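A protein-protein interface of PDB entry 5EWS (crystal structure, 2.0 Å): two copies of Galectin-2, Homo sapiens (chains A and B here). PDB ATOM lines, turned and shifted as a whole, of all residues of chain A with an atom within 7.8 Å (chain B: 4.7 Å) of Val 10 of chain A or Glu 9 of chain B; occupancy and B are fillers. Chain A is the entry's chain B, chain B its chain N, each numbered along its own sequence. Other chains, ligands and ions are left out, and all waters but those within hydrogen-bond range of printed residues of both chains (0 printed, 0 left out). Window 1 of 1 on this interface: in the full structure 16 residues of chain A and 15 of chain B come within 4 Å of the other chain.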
ATOM      1  N   GLU A   7     -11.376  11.984  23.312  1.00  0.00           N
ATOM      2  CA  GLU A   7     -10.046  12.501  23.636  1.00  0.00           C
ATOM      3  C   GLU A   7      -9.559  13.316  22.442  1.00  0.00           C
ATOM      4  O   GLU A   7      -8.777  12.859  21.605  1.00  0.00           O
ATOM      5  CB  GLU A   7      -9.090  11.365  23.976  1.00  0.00           C
ATOM      6  CG  GLU A   7      -9.361  10.695  25.314  1.00  0.00           C
ATOM      7  CD  GLU A   7      -8.269   9.719  25.706  1.00  0.00           C
ATOM      8  OE1 GLU A   7      -7.464   9.343  24.828  1.00  0.00           O
ATOM      9  OE2 GLU A   7      -8.211   9.333  26.893  1.00  0.00           O
ATOM     10  N   LEU A   8     -10.035  14.558  22.383  1.00  0.00           N
ATOM     11  CA  LEU A   8      -9.839  15.398  21.208  1.00  0.00           C
ATOM     12  C   LEU A   8      -8.361  15.652  20.932  1.00  0.00           C
ATOM     13  O   LEU A   8      -7.556  15.830  21.851  1.00  0.00           O
ATOM     14  CB  LEU A   8     -10.580  16.723  21.388  1.00  0.00           C
ATOM     15  CG  LEU A   8     -11.967  16.804  20.745  1.00  0.00           C
ATOM     16  CD1 LEU A   8     -12.950  15.876  21.442  1.00  0.00           C
ATOM     17  CD2 LEU A   8     -12.485  18.233  20.758  1.00  0.00           C
ATOM     18  N   GLU A   9      -8.014  15.671  19.646  1.00  0.00           N
ATOM     19  CA  GLU A   9      -6.701  16.072  19.160  1.00  0.00           C
ATOM     20  C   GLU A   9      -6.848  17.207  18.162  1.00  0.00           C
ATOM     21  O   GLU A   9      -7.687  17.135  17.259  1.00  0.00           O
ATOM     22  CB  GLU A   9      -5.967  14.919  18.471  1.00  0.00           C
ATOM     23  CG  GLU A   9      -5.207  13.980  19.371  1.00  0.00           C
ATOM     24  CD  GLU A   9      -4.317  13.042  18.574  1.00  0.00           C
ATOM     25  OE1 GLU A   9      -4.852  12.290  17.732  1.00  0.00           O
ATOM     26  OE2 GLU A   9      -3.085  13.066  18.777  1.00  0.00           O
ATOM     27  N   VAL A  10      -6.045  18.252  18.328  1.00  0.00           N
ATOM     28  CA  VAL A  10      -5.983  19.356  17.381  1.00  0.00           C
ATOM     29  C   VAL A  10      -4.563  19.403  16.833  1.00  0.00           C
ATOM     30  O   VAL A  10      -3.607  19.617  17.588  1.00  0.00           O
ATOM     31  CB  VAL A  10      -6.378  20.693  18.025  1.00  0.00           C
ATOM     32  CG1 VAL A  10      -6.471  21.773  16.968  1.00  0.00           C
ATOM     33  CG2 VAL A  10      -7.705  20.553  18.753  1.00  0.00           C
ATOM     34  N   LYS A  11      -4.425  19.185  15.526  1.00  0.00           N
ATOM     35  CA  LYS A  11      -3.128  19.098  14.872  1.00  0.00           C
ATOM     36  C   LYS A  11      -2.962  20.232  13.870  1.00  0.00           C
ATOM     37  O   LYS A  11      -3.939  20.724  13.299  1.00  0.00           O
ATOM     38  CB  LYS A  11      -2.956  17.758  14.147  1.00  0.00           C
ATOM     39  CG  LYS A  11      -2.922  16.539  15.052  1.00  0.00           C
ATOM     40  CD  LYS A  11      -3.039  15.265  14.230  1.00  0.00           C
ATOM     41  CE  LYS A  11      -2.697  14.031  15.048  1.00  0.00           C
ATOM     42  NZ  LYS A  11      -1.247  13.968  15.379  1.00  0.00           N
ATOM     43  N   ASN A  12      -1.704  20.631  13.660  1.00  0.00           N
ATOM     44  CA  ASN A  12      -1.332  21.645  12.671  1.00  0.00           C
ATOM     45  C   ASN A  12      -1.889  23.024  13.022  1.00  0.00           C
ATOM     46  O   ASN A  12      -2.260  23.797  12.139  1.00  0.00           O
ATOM     47  CB  ASN A  12      -1.748  21.242  11.253  1.00  0.00           C
ATOM     48  CG  ASN A  12      -1.259  19.861  10.874  1.00  0.00           C
ATOM     49  OD1 ASN A  12      -0.119  19.496  11.157  1.00  0.00           O
ATOM     50  ND2 ASN A  12      -2.119  19.087  10.225  1.00  0.00           N
ATOM     51  N   MET A  13      -1.949  23.335  14.313  1.00  0.00           N
ATOM     52  CA  MET A  13      -2.212  24.710  14.697  1.00  0.00           C
ATOM     53  C   MET A  13      -0.994  25.565  14.376  1.00  0.00           C
ATOM     54  O   MET A  13       0.094  25.066  14.076  1.00  0.00           O
ATOM     55  CB  MET A  13      -2.527  24.828  16.187  1.00  0.00           C
ATOM     56  CG  MET A  13      -3.545  23.851  16.711  1.00  0.00           C
ATOM     57  SD  MET A  13      -3.862  24.158  18.457  1.00  0.00           S
ATOM     58  CE  MET A  13      -2.212  23.992  19.130  1.00  0.00           C
ATOM     59  N   ASP A  14      -1.179  26.872  14.445  1.00  0.00           N
ATOM     60  CA  ASP A  14      -0.087  27.808  14.255  1.00  0.00           C
ATOM     61  C   ASP A  14      -0.162  28.804  15.413  1.00  0.00           C
ATOM     62  O   ASP A  14      -0.568  29.959  15.268  1.00  0.00           O
ATOM     63  CB  ASP A  14      -0.163  28.461  12.871  1.00  0.00           C
ATOM     64  CG  ASP A  14       1.125  29.148  12.476  1.00  0.00           C
ATOM     65  OD1 ASP A  14       2.165  28.866  13.103  1.00  0.00           O
ATOM     66  OD2 ASP A  14       1.116  29.902  11.481  1.00  0.00           O
ATOM     67  N   LEU A  21      -4.516  30.922  23.752  1.00  0.00           N
ATOM     68  CA  LEU A  21      -5.410  29.810  23.461  1.00  0.00           C
ATOM     69  C   LEU A  21      -6.417  29.686  24.593  1.00  0.00           C
ATOM     70  O   LEU A  21      -6.037  29.427  25.740  1.00  0.00           O
ATOM     71  CB  LEU A  21      -4.628  28.508  23.282  1.00  0.00           C
ATOM     72  CG  LEU A  21      -5.426  27.206  23.207  1.00  0.00           C
ATOM     73  CD1 LEU A  21      -6.379  27.219  22.028  1.00  0.00           C
ATOM     74  CD2 LEU A  21      -4.482  26.017  23.116  1.00  0.00           C
ATOM     75  N   ILE A  23      -9.610  27.675  26.034  1.00  0.00           N
ATOM     76  CA  ILE A  23     -10.246  26.365  25.956  1.00  0.00           C
ATOM     77  C   ILE A  23     -11.405  26.318  26.941  1.00  0.00           C
ATOM     78  O   ILE A  23     -11.245  26.669  28.115  1.00  0.00           O
ATOM     79  CB  ILE A  23      -9.250  25.223  26.231  1.00  0.00           C
ATOM     80  CG1 ILE A  23      -8.191  25.155  25.128  1.00  0.00           C
ATOM     81  CG2 ILE A  23      -9.980  23.894  26.359  1.00  0.00           C
ATOM     82  CD1 ILE A  23      -7.199  24.026  25.302  1.00  0.00           C
ATOM     83  N   ASN A  37      -2.695  18.902  26.854  1.00  0.00           N
ATOM     84  CA  ASN A  37      -1.326  18.854  26.354  1.00  0.00           C
ATOM     85  C   ASN A  37      -1.125  19.835  25.205  1.00  0.00           C
ATOM     86  O   ASN A  37      -1.977  19.956  24.322  1.00  0.00           O
ATOM     87  CB  ASN A  37      -0.956  17.442  25.893  1.00  0.00           C
ATOM     88  CG  ASN A  37      -0.794  16.476  27.049  1.00  0.00           C
ATOM     89  OD1 ASN A  37      -0.216  16.818  28.080  1.00  0.00           O
ATOM     90  ND2 ASN A  37      -1.298  15.260  26.879  1.00  0.00           N
ATOM     91  N   LEU A  38       0.015  20.529  25.224  1.00  0.00           N
ATOM     92  CA  LEU A  38       0.348  21.538  24.227  1.00  0.00           C
ATOM     93  C   LEU A  38       1.827  21.441  23.878  1.00  0.00           C
ATOM     94  O   LEU A  38       2.676  21.443  24.774  1.00  0.00           O
ATOM     95  CB  LEU A  38       0.006  22.940  24.744  1.00  0.00           C
ATOM     96  CG  LEU A  38       0.037  24.106  23.760  1.00  0.00           C
ATOM     97  CD1 LEU A  38      -0.844  23.817  22.563  1.00  0.00           C
ATOM     98  CD2 LEU A  38      -0.425  25.370  24.464  1.00  0.00           C
ATOM     99  N   GLY A  39       2.133  21.361  22.582  1.00  0.00           N
ATOM    100  CA  GLY A  39       3.506  21.185  22.138  1.00  0.00           C
ATOM    101  C   GLY A  39       3.678  21.015  20.640  1.00  0.00           C
ATOM    102  O   GLY A  39       2.922  21.587  19.850  1.00  0.00           O
ATOM    103  N   LEU A 117       3.733  26.412  18.529  1.00  0.00           N
ATOM    104  CA  LEU A 117       2.959  25.281  19.022  1.00  0.00           C
ATOM    105  C   LEU A 117       1.937  24.852  17.978  1.00  0.00           C
ATOM    106  O   LEU A 117       1.140  25.670  17.508  1.00  0.00           O
ATOM    107  CB  LEU A 117       2.254  25.655  20.324  1.00  0.00           C
ATOM    108  CG  LEU A 117       3.161  26.231  21.410  1.00  0.00           C
ATOM    109  CD1 LEU A 117       2.322  26.671  22.583  1.00  0.00           C
ATOM    110  CD2 LEU A 117       4.203  25.213  21.842  1.00  0.00           C
ATOM    111  N   SER A 118       1.961  23.567  17.618  1.00  0.00           N
ATOM    112  CA  SER A 118       1.087  23.044  16.580  1.00  0.00           C
ATOM    113  C   SER A 118       0.150  21.939  17.044  1.00  0.00           C
ATOM    114  O   SER A 118      -0.720  21.531  16.266  1.00  0.00           O
ATOM    115  CB  SER A 118       1.916  22.516  15.399  1.00  0.00           C
ATOM    116  OG  SER A 118       2.758  21.451  15.805  1.00  0.00           O
ATOM    117  N   TYR A 119       0.288  21.447  18.273  1.00  0.00           N
ATOM    118  CA  TYR A 119      -0.373  20.217  18.693  1.00  0.00           C
ATOM    119  C   TYR A 119      -1.084  20.433  20.019  1.00  0.00           C
ATOM    120  O   TYR A 119      -0.490  20.946  20.972  1.00  0.00           O
ATOM    121  CB  TYR A 119       0.632  19.067  18.814  1.00  0.00           C
ATOM    122  CG  TYR A 119       0.022  17.764  19.282  1.00  0.00           C
ATOM    123  CD1 TYR A 119      -0.584  16.896  18.384  1.00  0.00           C
ATOM    124  CD2 TYR A 119       0.059  17.399  20.623  1.00  0.00           C
ATOM    125  CE1 TYR A 119      -1.143  15.706  18.808  1.00  0.00           C
ATOM    126  CE2 TYR A 119      -0.497  16.211  21.055  1.00  0.00           C
ATOM    127  CZ  TYR A 119      -1.096  15.368  20.144  1.00  0.00           C
ATOM    128  OH  TYR A 119      -1.649  14.183  20.572  1.00  0.00           O
ATOM    129  N   LEU A 120      -2.353  20.035  20.075  1.00  0.00           N
ATOM    130  CA  LEU A 120      -3.142  20.077  21.298  1.00  0.00           C
ATOM    131  C   LEU A 120      -3.901  18.768  21.445  1.00  0.00           C
ATOM    132  O   LEU A 120      -4.512  18.292  20.484  1.00  0.00           O
ATOM    133  CB  LEU A 120      -4.114  21.264  21.279  1.00  0.00           C
ATOM    134  CG  LEU A 120      -5.271  21.292  22.279  1.00  0.00           C
ATOM    135  CD1 LEU A 120      -4.769  21.429  23.705  1.00  0.00           C
ATOM    136  CD2 LEU A 120      -6.220  22.427  21.938  1.00  0.00           C
ATOM    137  N   SER A 121      -3.859  18.185  22.642  1.00  0.00           N
ATOM    138  CA  SER A 121      -4.588  16.958  22.927  1.00  0.00           C
ATOM    139  C   SER A 121      -5.153  17.035  24.337  1.00  0.00           C
ATOM    140  O   SER A 121      -4.545  17.623  25.235  1.00  0.00           O
ATOM    141  CB  SER A 121      -3.699  15.714  22.778  1.00  0.00           C
ATOM    142  OG  SER A 121      -2.753  15.626  23.828  1.00  0.00           O
ATOM    143  N   VAL A 122      -6.318  16.423  24.525  1.00  0.00           N
ATOM    144  CA  VAL A 122      -7.000  16.391  25.813  1.00  0.00           C
ATOM    145  C   VAL A 122      -7.242  14.941  26.211  1.00  0.00           C
ATOM    146  O   VAL A 122      -7.675  14.126  25.388  1.00  0.00           O
ATOM    147  CB  VAL A 122      -8.325  17.179  25.766  1.00  0.00           C
ATOM    148  CG1 VAL A 122      -9.127  16.948  27.032  1.00  0.00           C
ATOM    149  CG2 VAL A 122      -8.047  18.661  25.570  1.00  0.00           C
ATOM    150  N   MET A 128     -13.651  18.623  25.768  1.00  0.00           N
ATOM    151  CA  MET A 128     -13.491  19.964  25.226  1.00  0.00           C
ATOM    152  C   MET A 128     -14.630  20.288  24.272  1.00  0.00           C
ATOM    153  O   MET A 128     -14.916  19.525  23.342  1.00  0.00           O
ATOM    154  CB  MET A 128     -12.148  20.100  24.514  1.00  0.00           C
ATOM    155  CG  MET A 128     -11.930  21.468  23.887  1.00  0.00           C
ATOM    156  SD  MET A 128     -10.253  21.695  23.270  1.00  0.00           S
ATOM    157  CE  MET A 128      -9.926  20.095  22.539  1.00  0.00           C
ATOM    158  N   PHE A 131     -12.451  25.762  21.436  1.00  0.00           N
ATOM    159  CA  PHE A 131     -11.214  26.494  21.670  1.00  0.00           C
ATOM    160  C   PHE A 131     -11.174  27.670  20.704  1.00  0.00           C
ATOM    161  O   PHE A 131     -11.870  27.689  19.687  1.00  0.00           O
ATOM    162  CB  PHE A 131      -9.933  25.633  21.541  1.00  0.00           C
ATOM    163  CG  PHE A 131      -9.433  25.425  20.124  1.00  0.00           C
ATOM    164  CD1 PHE A 131      -8.676  26.403  19.487  1.00  0.00           C
ATOM    165  CD2 PHE A 131      -9.631  24.225  19.471  1.00  0.00           C
ATOM    166  CE1 PHE A 131      -8.196  26.213  18.207  1.00  0.00           C
ATOM    167  CE2 PHE A 131      -9.144  24.027  18.186  1.00  0.00           C
ATOM    168  CZ  PHE A 131      -8.426  25.023  17.557  1.00  0.00           C
ATOM    169  N   GLU B   7      -3.343  24.045   8.388  1.00  0.00           N
ATOM    170  CA  GLU B   7      -4.369  23.165   7.835  1.00  0.00           C
ATOM    171  C   GLU B   7      -4.814  22.215   8.943  1.00  0.00           C
ATOM    172  O   GLU B   7      -4.373  21.068   9.056  1.00  0.00           O
ATOM    173  CB  GLU B   7      -3.836  22.439   6.608  1.00  0.00           C
ATOM    174  CG  GLU B   7      -3.633  23.377   5.423  1.00  0.00           C
ATOM    175  CD  GLU B   7      -3.291  22.657   4.136  1.00  0.00           C
ATOM    176  OE1 GLU B   7      -3.360  23.297   3.065  1.00  0.00           O
ATOM    177  OE2 GLU B   7      -2.934  21.463   4.193  1.00  0.00           O
ATOM    178  N   LEU B   8      -5.704  22.736   9.785  1.00  0.00           N
ATOM    179  CA  LEU B   8      -6.109  22.066  11.012  1.00  0.00           C
ATOM    180  C   LEU B   8      -6.787  20.734  10.727  1.00  0.00           C
ATOM    181  O   LEU B   8      -7.549  20.600   9.767  1.00  0.00           O
ATOM    182  CB  LEU B   8      -7.084  22.960  11.780  1.00  0.00           C
ATOM    183  CG  LEU B   8      -6.623  23.904  12.889  1.00  0.00           C
ATOM    184  CD1 LEU B   8      -7.826  24.393  13.681  1.00  0.00           C
ATOM    185  CD2 LEU B   8      -5.621  23.243  13.799  1.00  0.00           C
ATOM    186  N   GLU B   9      -6.483  19.733  11.550  1.00  0.00           N
ATOM    187  CA  GLU B   9      -7.284  18.519  11.614  1.00  0.00           C
ATOM    188  C   GLU B   9      -7.630  18.256  13.072  1.00  0.00           C
ATOM    189  O   GLU B   9      -6.756  18.321  13.943  1.00  0.00           O
ATOM    190  CB  GLU B   9      -6.611  17.302  10.967  1.00  0.00           C
ATOM    191  CG  GLU B   9      -5.199  16.975  11.369  1.00  0.00           C
ATOM    192  CD  GLU B   9      -4.734  15.701  10.688  1.00  0.00           C
ATOM    193  OE1 GLU B   9      -5.540  15.114   9.932  1.00  0.00           O
ATOM    194  OE2 GLU B   9      -3.583  15.274  10.912  1.00  0.00           O
ATOM    195  N   VAL B  10      -8.900  17.957  13.336  1.00  0.00           N
ATOM    196  CA  VAL B  10      -9.382  17.651  14.679  1.00  0.00           C
ATOM    197  C   VAL B  10      -9.826  16.198  14.696  1.00  0.00           C
ATOM    198  O   VAL B  10     -10.695  15.795  13.912  1.00  0.00           O
ATOM    199  CB  VAL B  10     -10.530  18.582  15.099  1.00  0.00           C
ATOM    200  CG1 VAL B  10     -10.895  18.352  16.559  1.00  0.00           C
ATOM    201  CG2 VAL B  10     -10.151  20.034  14.861  1.00  0.00           C
ATOM    202  N   LYS B  11      -9.222  15.412  15.580  1.00  0.00           N
ATOM    203  CA  LYS B  11      -9.472  13.985  15.670  1.00  0.00           C
ATOM    204  C   LYS B  11     -10.196  13.644  16.964  1.00  0.00           C
ATOM    205  O   LYS B  11     -10.204  14.416  17.927  1.00  0.00           O
ATOM    206  CB  LYS B  11      -8.167  13.187  15.593  1.00  0.00           C
ATOM    207  CG  LYS B  11      -7.382  13.364  14.309  1.00  0.00           C
ATOM    208  CD  LYS B  11      -6.141  12.487  14.338  1.00  0.00           C
ATOM    209  CE  LYS B  11      -5.717  12.058  12.946  1.00  0.00           C
ATOM    210  NZ  LYS B  11      -5.004  13.144  12.231  1.00  0.00           N
ATOM    211  N   TYR B 119     -13.754  13.243  12.803  1.00  0.00           N
ATOM    212  CA  TYR B 119     -12.636  13.810  12.064  1.00  0.00           C
ATOM    213  C   TYR B 119     -13.064  15.101  11.387  1.00  0.00           C
ATOM    214  O   TYR B 119     -14.009  15.110  10.593  1.00  0.00           O
ATOM    215  CB  TYR B 119     -12.121  12.819  11.018  1.00  0.00           C
ATOM    216  CG  TYR B 119     -10.988  13.349  10.172  1.00  0.00           C
ATOM    217  CD1 TYR B 119      -9.678  13.294  10.621  1.00  0.00           C
ATOM    218  CD2 TYR B 119     -11.231  13.902   8.921  1.00  0.00           C
ATOM    219  CE1 TYR B 119      -8.640  13.777   9.853  1.00  0.00           C
ATOM    220  CE2 TYR B 119     -10.199  14.387   8.144  1.00  0.00           C
ATOM    221  CZ  TYR B 119      -8.906  14.322   8.617  1.00  0.00           C
ATOM    222  OH  TYR B 119      -7.865  14.799   7.855  1.00  0.00           O
ATOM    223  N   LEU B 120     -12.308  16.163  11.636  1.00  0.00           N
ATOM    224  CA  LEU B 120     -12.509  17.452  10.995  1.00  0.00           C
ATOM    225  C   LEU B 120     -11.153  17.920  10.513  1.00  0.00           C
ATOM    226  O   LEU B 120     -10.181  17.876  11.270  1.00  0.00           O
ATOM    227  CB  LEU B 120     -13.116  18.478  11.961  1.00  0.00           C
ATOM    228  CG  LEU B 120     -13.028  19.956  11.559  1.00  0.00           C
ATOM    229  CD1 LEU B 120     -13.869  20.258  10.327  1.00  0.00           C
ATOM    230  CD2 LEU B 120     -13.424  20.864  12.718  1.00  0.00           C
ATOM    231  N   SER B 121     -11.084  18.359   9.262  1.00  0.00           N
ATOM    232  CA  SER B 121      -9.837  18.851   8.704  1.00  0.00           C
ATOM    233  C   SER B 121     -10.128  20.047   7.814  1.00  0.00           C
ATOM    234  O   SER B 121     -11.183  20.133   7.183  1.00  0.00           O
ATOM    235  CB  SER B 121      -9.092  17.769   7.911  1.00  0.00           C
ATOM    236  OG  SER B 121      -9.742  17.482   6.688  1.00  0.00           O
ATOM    237  N   ARG B 123      -8.400  22.460   4.719  1.00  0.00           N
ATOM    238  CA  ARG B 123      -7.403  22.546   3.667  1.00  0.00           C
ATOM    239  C   ARG B 123      -7.474  23.918   3.009  1.00  0.00           C
ATOM    240  O   ARG B 123      -8.440  24.666   3.182  1.00  0.00           O
ATOM    241  CB  ARG B 123      -7.610  21.445   2.618  1.00  0.00           C
ATOM    242  CG  ARG B 123      -7.714  20.043   3.199  1.00  0.00           C
ATOM    243  CD  ARG B 123      -6.343  19.423   3.408  1.00  0.00           C
ATOM    244  NE  ARG B 123      -6.420  18.143   4.103  1.00  0.00           N
ATOM    245  CZ  ARG B 123      -6.369  18.005   5.423  1.00  0.00           C
ATOM    246  NH1 ARG B 123      -6.233  19.072   6.200  1.00  0.00           N
ATOM    247  NH2 ARG B 123      -6.446  16.800   5.970  1.00  0.00           N
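N of Met 13 of chain A lies within hydrogen-bond range of O of Ser 118 of chain A, at 2.9 Å.
The backbone NH (N) of Val 10 of chain B lies within hydrogen-bond range of the backbone carbonyl oxygen (O) of Leu 120 of chain B (2.4 Å).
The side-chain amino group (NZ) of Lys 11 of chain A lies within salt-bridge range of the side-chain carboxylate (OE2) of Glu 9 of chain A (3.97 Å).
The side-chain hydroxyl (OH) of Tyr 119 of chain A lies within hydrogen-bond range of the side-chain carboxylate (OE2) of Glu 9 of chain A (2.6 Å).
O of Leu 120 of chain A is in hydrogen-bond range of N of Val 10 of chain A (2.6 Å).
The side-chain hydroxyl of Tyr 119 of chain B sits at hydrogen-bond distance from the side-chain carboxylate of Glu 9 of chain B, 3.1 Å away.
Printed residues of chain B that touch a printed residue of chain A: Glu 7, Leu 8, Glu 9, Val 10 and Lys 11.
Hydrophobic or aromatic side chains of chain B within 4 Å of the printed part of chain A: Leu 8 and Val 10.
Of the 21 printed residues of chain A, 7 touch a printed residue of chain B.
Hydrophobic or aromatic side chains of chain A that line the printed part of chain B: Val 10, Met 13 and Phe 131.
Among the printed residues, 14 pairs touch across the chains.
Among the printed residues, no Asp or Glu carboxylate lies within 4 Å of a Lys or Arg side-chain nitrogen of the other chain.
Printed residues of chain B within 4 Å of Lys 11 of chain A: Leu 8, Glu 9 and Lys 11.
Printed residues of chain A within 4 Å of Leu 8 of chain B: Val 10, Lys 11, Asn 12, Met 13 and Phe 131.
Printed residues of chain B within 4 Å of Phe 131 of chain A: Leu 8.
Tyr 119 of chain B touches none of the printed residues of chain A.
Arg 123 of chain B touches none of the printed residues of chain A.
The nearest residue of chain A that does not touch Glu 9 of chain B is Met 13 of chain A (6.4 Å).
Among the printed residues, merely in contact across the chains: Lys 11 of chain A with Leu 8 of chain B (3.1 Å), Glu 9 of chain A with Val 10 of chain B (3.1 Å), Leu 8 of chain A with Lys 11 of chain B (3.4 Å), Lys 11 of chain A with Lys 11 of chain B (3.5 Å), Val 10 of chain A with Leu 8 of chain B (3.6 Å), Met 13 of chain A with Leu 8 of chain B (3.6 Å), Glu 9 of chain A with Glu 9 of chain B (3.6 Å), Val 10 of chain A with Glu 9 of chain B (3.7 Å), Asn 12 of chain A with Leu 8 of chain B (3.8 Å), Asn 12 of chain A with Glu 9 of chain B (3.9 Å) and Phe 131 of chain A with Leu 8 of chain B (3.97 Å).
Leu 8 of chain A touches Lys 11 of chain B, and with the chains exchanged Lys 11 of chain A touches Leu 8 of chain B.
Glu 9 of chain B touches its own counterpart, Glu 9 of chain A.
Val 10 of chain A touches Leu 8 of chain B, but with the chains exchanged Leu 8 of chain A does not touch Val 10 of chain B (4.5 Å).
Lys 11 of chain B touches its own counterpart, Lys 11 of chain A.
Positions printed for both chains: 7, 8, 9, 10, 11, 119, 120 and 121.
Of the 14 pairs that touch across the chains among the printed residues, 8 have their exchanged pair printed and touching as well.
ND2 of Asn 12 of chain A sits at hydrogen-bond distance from O of Glu 7 of chain B.
The backbone NH of Lys 11 of chain A sits at hydrogen-bond distance from the backbone carbonyl oxygen of Glu 9 of chain B.
The backbone carbonyl oxygen (O) of Glu 9 of chain A is in hydrogen-bond range of the backbone NH (N) of Lys 11 of chain B (2.9 Å).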
